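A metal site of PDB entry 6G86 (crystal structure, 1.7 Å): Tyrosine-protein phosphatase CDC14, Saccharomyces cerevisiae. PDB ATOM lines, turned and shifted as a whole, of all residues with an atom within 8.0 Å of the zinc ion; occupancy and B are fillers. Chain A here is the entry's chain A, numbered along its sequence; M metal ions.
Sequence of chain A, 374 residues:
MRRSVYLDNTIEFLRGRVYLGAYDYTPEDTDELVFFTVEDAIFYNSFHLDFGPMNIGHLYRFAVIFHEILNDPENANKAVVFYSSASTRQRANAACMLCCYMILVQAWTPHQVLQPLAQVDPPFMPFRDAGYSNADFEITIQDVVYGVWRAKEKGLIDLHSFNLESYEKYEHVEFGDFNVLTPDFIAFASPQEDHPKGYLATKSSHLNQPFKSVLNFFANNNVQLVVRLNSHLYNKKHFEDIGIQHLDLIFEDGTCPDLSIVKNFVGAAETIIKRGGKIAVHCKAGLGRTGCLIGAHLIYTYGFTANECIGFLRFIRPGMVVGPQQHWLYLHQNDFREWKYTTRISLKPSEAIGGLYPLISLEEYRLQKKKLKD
Merely in contact with the zinc ion: Leu 207 (3.99 Å). The nearest printed residue that does not touch the zinc ion is Pro 196 (4.3 Å).
The side-chain carboxylate of Glu 193 sits at hydrogen-bond distance from the backbone NH of Asn 235, at 2.9 Å.
The zinc ion is bound by OE1 of Glu 193, NE2 of His 238, ND1 of His 195 and NE2 of His 206. Slightly farther from the zinc ion lies OE2 of Glu 193 (2.8 Å).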
ATOM      1  N   GLN A 192     -14.325 -15.117  11.236  1.00  0.00           N
ATOM      2  CA  GLN A 192     -15.316 -14.722  10.246  1.00  0.00           C
ATOM      3  C   GLN A 192     -14.770 -13.517   9.503  1.00  0.00           C
ATOM      4  O   GLN A 192     -14.079 -12.682  10.088  1.00  0.00           O
ATOM      5  CB  GLN A 192     -16.652 -14.341  10.902  1.00  0.00           C
ATOM      6  CG  GLN A 192     -17.300 -15.469  11.697  1.00  0.00           C
ATOM      7  CD  GLN A 192     -18.525 -14.989  12.441  1.00  0.00           C
ATOM      8  OE1 GLN A 192     -19.477 -14.512  11.846  1.00  0.00           O
ATOM      9  NE2 GLN A 192     -18.494 -15.104  13.763  1.00  0.00           N
ATOM     10  N   GLU A 193     -15.112 -13.406   8.219  1.00  0.00           N
ATOM     11  CA  GLU A 193     -14.690 -12.228   7.464  1.00  0.00           C
ATOM     12  C   GLU A 193     -15.597 -12.039   6.270  1.00  0.00           C
ATOM     13  O   GLU A 193     -16.378 -12.912   5.898  1.00  0.00           O
ATOM     14  CB  GLU A 193     -13.244 -12.378   6.980  1.00  0.00           C
ATOM     15  CG  GLU A 193     -13.071 -13.493   5.992  1.00  0.00           C
ATOM     16  CD  GLU A 193     -11.814 -13.331   5.139  1.00  0.00           C
ATOM     17  OE1 GLU A 193     -11.462 -12.172   4.768  1.00  0.00           O
ATOM     18  OE2 GLU A 193     -11.201 -14.365   4.834  1.00  0.00           O
ATOM     19  N   ASP A 194     -15.489 -10.860   5.672  1.00  0.00           N
ATOM     20  CA  ASP A 194     -16.025 -10.630   4.334  1.00  0.00           C
ATOM     21  C   ASP A 194     -14.816 -10.424   3.426  1.00  0.00           C
ATOM     22  O   ASP A 194     -14.187  -9.366   3.425  1.00  0.00           O
ATOM     23  CB  ASP A 194     -17.014  -9.480   4.320  1.00  0.00           C
ATOM     24  CG  ASP A 194     -18.360  -9.886   4.872  1.00  0.00           C
ATOM     25  OD1 ASP A 194     -19.109 -10.621   4.188  1.00  0.00           O
ATOM     26  OD2 ASP A 194     -18.674  -9.501   6.010  1.00  0.00           O
ATOM     27  N   HIS A 195     -14.474 -11.491   2.701  1.00  0.00           N
ATOM     28  CA  HIS A 195     -13.278 -11.486   1.866  1.00  0.00           C
ATOM     29  C   HIS A 195     -13.601 -10.794   0.538  1.00  0.00           C
ATOM     30  O   HIS A 195     -14.566 -11.168  -0.125  1.00  0.00           O
ATOM     31  CB  HIS A 195     -12.801 -12.913   1.610  1.00  0.00           C
ATOM     32  CG  HIS A 195     -11.443 -12.990   0.984  1.00  0.00           C
ATOM     33  ND1 HIS A 195     -10.279 -12.811   1.707  1.00  0.00           N
ATOM     34  CD2 HIS A 195     -11.069 -13.219  -0.299  1.00  0.00           C
ATOM     35  CE1 HIS A 195      -9.244 -12.924   0.891  1.00  0.00           C
ATOM     36  NE2 HIS A 195      -9.696 -13.160  -0.329  1.00  0.00           N
ATOM     37  N   PRO A 196     -12.828  -9.793   0.139  1.00  0.00           N
ATOM     38  CA  PRO A 196     -13.253  -8.946  -0.983  1.00  0.00           C
ATOM     39  C   PRO A 196     -13.331  -9.738  -2.284  1.00  0.00           C
ATOM     40  O   PRO A 196     -12.522 -10.642  -2.528  1.00  0.00           O
ATOM     41  CB  PRO A 196     -12.173  -7.856  -1.051  1.00  0.00           C
ATOM     42  CG  PRO A 196     -11.556  -7.853   0.322  1.00  0.00           C
ATOM     43  CD  PRO A 196     -11.606  -9.288   0.778  1.00  0.00           C
ATOM     44  N   SER A 205      -8.106  -3.261   3.362  1.00  0.00           N
ATOM     45  CA  SER A 205      -7.605  -4.120   4.432  1.00  0.00           C
ATOM     46  C   SER A 205      -8.761  -4.519   5.339  1.00  0.00           C
ATOM     47  O   SER A 205      -9.175  -3.768   6.215  1.00  0.00           O
ATOM     48  CB  SER A 205      -6.510  -3.410   5.227  1.00  0.00           C
ATOM     49  OG  SER A 205      -5.691  -4.349   5.892  1.00  0.00           O
ATOM     50  N   HIS A 206      -9.240  -5.740   5.144  1.00  0.00           N
ATOM     51  CA  HIS A 206     -10.615  -6.088   5.487  1.00  0.00           C
ATOM     52  C   HIS A 206     -10.756  -6.987   6.710  1.00  0.00           C
ATOM     53  O   HIS A 206     -11.887  -7.263   7.117  1.00  0.00           O
ATOM     54  CB  HIS A 206     -11.256  -6.813   4.306  1.00  0.00           C
ATOM     55  CG  HIS A 206     -10.498  -8.037   3.890  1.00  0.00           C
ATOM     56  ND1 HIS A 206      -9.336  -7.987   3.155  1.00  0.00           N
ATOM     57  CD2 HIS A 206     -10.706  -9.349   4.173  1.00  0.00           C
ATOM     58  CE1 HIS A 206      -8.888  -9.207   2.952  1.00  0.00           C
ATOM     59  NE2 HIS A 206      -9.692 -10.054   3.572  1.00  0.00           N
ATOM     60  N   LEU A 207      -9.665  -7.475   7.296  1.00  0.00           N
ATOM     61  CA  LEU A 207      -9.806  -8.405   8.416  1.00  0.00           C
ATOM     62  C   LEU A 207     -10.259  -7.675   9.672  1.00  0.00           C
ATOM     63  O   LEU A 207      -9.827  -6.540   9.950  1.00  0.00           O
ATOM     64  CB  LEU A 207      -8.474  -9.122   8.659  1.00  0.00           C
ATOM     65  CG  LEU A 207      -7.989  -9.994   7.510  1.00  0.00           C
ATOM     66  CD1 LEU A 207      -6.556 -10.439   7.759  1.00  0.00           C
ATOM     67  CD2 LEU A 207      -8.902 -11.198   7.323  1.00  0.00           C
ATOM     68  N   ASN A 208     -11.135  -8.311  10.446  1.00  0.00           N
ATOM     69  CA  ASN A 208     -11.587  -7.705  11.692  1.00  0.00           C
ATOM     70  C   ASN A 208     -10.590  -7.971  12.806  1.00  0.00           C
ATOM     71  O   ASN A 208      -9.650  -8.754  12.673  1.00  0.00           O
ATOM     72  CB  ASN A 208     -13.001  -8.201  12.081  1.00  0.00           C
ATOM     73  CG  ASN A 208     -13.089  -9.735  12.265  1.00  0.00           C
ATOM     74  OD1 ASN A 208     -12.120 -10.418  12.606  1.00  0.00           O
ATOM     75  ND2 ASN A 208     -14.298 -10.257  12.076  1.00  0.00           N
ATOM     76  N   PHE A 211      -9.926 -11.613  14.006  1.00  0.00           N
ATOM     77  CA  PHE A 211      -9.166 -12.429  13.065  1.00  0.00           C
ATOM     78  C   PHE A 211      -7.684 -12.039  13.093  1.00  0.00           C
ATOM     79  O   PHE A 211      -6.796 -12.905  13.105  1.00  0.00           O
ATOM     80  CB  PHE A 211      -9.755 -12.253  11.651  1.00  0.00           C
ATOM     81  CG  PHE A 211      -9.542 -13.402  10.725  1.00  0.00           C
ATOM     82  CD1 PHE A 211      -8.604 -14.373  10.988  1.00  0.00           C
ATOM     83  CD2 PHE A 211     -10.298 -13.486   9.548  1.00  0.00           C
ATOM     84  CE1 PHE A 211      -8.409 -15.431  10.080  1.00  0.00           C
ATOM     85  CE2 PHE A 211     -10.126 -14.542   8.639  1.00  0.00           C
ATOM     86  CZ  PHE A 211      -9.183 -15.509   8.890  1.00  0.00           C
ATOM     87  N   TYR A 234     -14.629 -18.056   6.399  1.00  0.00           N
ATOM     88  CA  TYR A 234     -13.491 -17.208   6.043  1.00  0.00           C
ATOM     89  C   TYR A 234     -12.721 -17.920   4.937  1.00  0.00           C
ATOM     90  O   TYR A 234     -12.892 -19.130   4.720  1.00  0.00           O
ATOM     91  CB  TYR A 234     -12.574 -16.950   7.254  1.00  0.00           C
ATOM     92  CG  TYR A 234     -11.969 -18.254   7.770  1.00  0.00           C
ATOM     93  CD1 TYR A 234     -12.632 -19.004   8.742  1.00  0.00           C
ATOM     94  CD2 TYR A 234     -10.765 -18.749   7.249  1.00  0.00           C
ATOM     95  CE1 TYR A 234     -12.098 -20.222   9.206  1.00  0.00           C
ATOM     96  CE2 TYR A 234     -10.228 -19.951   7.695  1.00  0.00           C
ATOM     97  CZ  TYR A 234     -10.895 -20.686   8.685  1.00  0.00           C
ATOM     98  OH  TYR A 234     -10.372 -21.897   9.099  1.00  0.00           O
ATOM     99  N   ASN A 235     -11.836 -17.167   4.293  1.00  0.00           N
ATOM    100  CA  ASN A 235     -10.922 -17.714   3.285  1.00  0.00           C
ATOM    101  C   ASN A 235      -9.642 -18.181   3.954  1.00  0.00           C
ATOM    102  O   ASN A 235      -8.928 -17.403   4.612  1.00  0.00           O
ATOM    103  CB  ASN A 235     -10.647 -16.652   2.209  1.00  0.00           C
ATOM    104  CG  ASN A 235      -9.921 -17.207   1.018  1.00  0.00           C
ATOM    105  OD1 ASN A 235      -8.929 -17.934   1.159  1.00  0.00           O
ATOM    106  ND2 ASN A 235     -10.414 -16.875  -0.187  1.00  0.00           N
ATOM    107  N   LYS A 236      -9.328 -19.474   3.786  1.00  0.00           N
ATOM    108  CA  LYS A 236      -8.156 -20.091   4.393  1.00  0.00           C
ATOM    109  C   LYS A 236      -6.845 -19.469   3.935  1.00  0.00           C
ATOM    110  O   LYS A 236      -5.815 -19.706   4.581  1.00  0.00           O
ATOM    111  CB  LYS A 236      -8.147 -21.587   4.060  1.00  0.00           C
ATOM    112  CG  LYS A 236      -7.812 -21.848   2.587  1.00  0.00           C
ATOM    113  CD  LYS A 236      -8.063 -23.269   2.192  1.00  0.00           C
ATOM    114  CE  LYS A 236      -7.625 -23.564   0.798  1.00  0.00           C
ATOM    115  NZ  LYS A 236      -6.160 -23.465   0.683  1.00  0.00           N
ATOM    116  N   LYS A 237      -6.838 -18.659   2.869  1.00  0.00           N
ATOM    117  CA  LYS A 237      -5.575 -18.121   2.391  1.00  0.00           C
ATOM    118  C   LYS A 237      -4.858 -17.293   3.458  1.00  0.00           C
ATOM    119  O   LYS A 237      -3.624 -17.191   3.438  1.00  0.00           O
ATOM    120  CB  LYS A 237      -5.806 -17.261   1.139  1.00  0.00           C
ATOM    121  CG  LYS A 237      -6.522 -15.952   1.439  1.00  0.00           C
ATOM    122  CD  LYS A 237      -6.271 -14.907   0.357  1.00  0.00           C
ATOM    123  CE  LYS A 237      -5.169 -13.961   0.770  1.00  0.00           C
ATOM    124  NZ  LYS A 237      -4.373 -13.498  -0.400  1.00  0.00           N
ATOM    125  N   HIS A 238      -5.614 -16.711   4.407  1.00  0.00           N
ATOM    126  CA  HIS A 238      -4.988 -15.868   5.417  1.00  0.00           C
ATOM    127  C   HIS A 238      -4.088 -16.680   6.356  1.00  0.00           C
ATOM    128  O   HIS A 238      -3.104 -16.158   6.880  1.00  0.00           O
ATOM    129  CB  HIS A 238      -6.070 -15.114   6.218  1.00  0.00           C
ATOM    130  CG  HIS A 238      -6.790 -14.090   5.388  1.00  0.00           C
ATOM    131  ND1 HIS A 238      -6.163 -12.948   4.920  1.00  0.00           N
ATOM    132  CD2 HIS A 238      -8.071 -14.020   4.947  1.00  0.00           C
ATOM    133  CE1 HIS A 238      -7.029 -12.225   4.223  1.00  0.00           C
ATOM    134  NE2 HIS A 238      -8.190 -12.855   4.228  1.00  0.00           N
ATOM    135  N   ASP A 241      -1.032 -17.568   4.164  1.00  0.00           N
ATOM    136  CA  ASP A 241      -0.211 -16.375   4.042  1.00  0.00           C
ATOM    137  C   ASP A 241       0.841 -16.275   5.147  1.00  0.00           C
ATOM    138  O   ASP A 241       1.866 -15.616   4.960  1.00  0.00           O
ATOM    139  CB  ASP A 241      -1.082 -15.116   4.083  1.00  0.00           C
ATOM    140  CG  ASP A 241      -1.781 -14.851   2.751  1.00  0.00           C
ATOM    141  OD1 ASP A 241      -1.473 -15.530   1.742  1.00  0.00           O
ATOM    142  OD2 ASP A 241      -2.665 -13.950   2.727  1.00  0.00           O
HETATM  143 ZN    ZN M   1      -9.958 -12.142   3.593  1.00  0.00          ZN
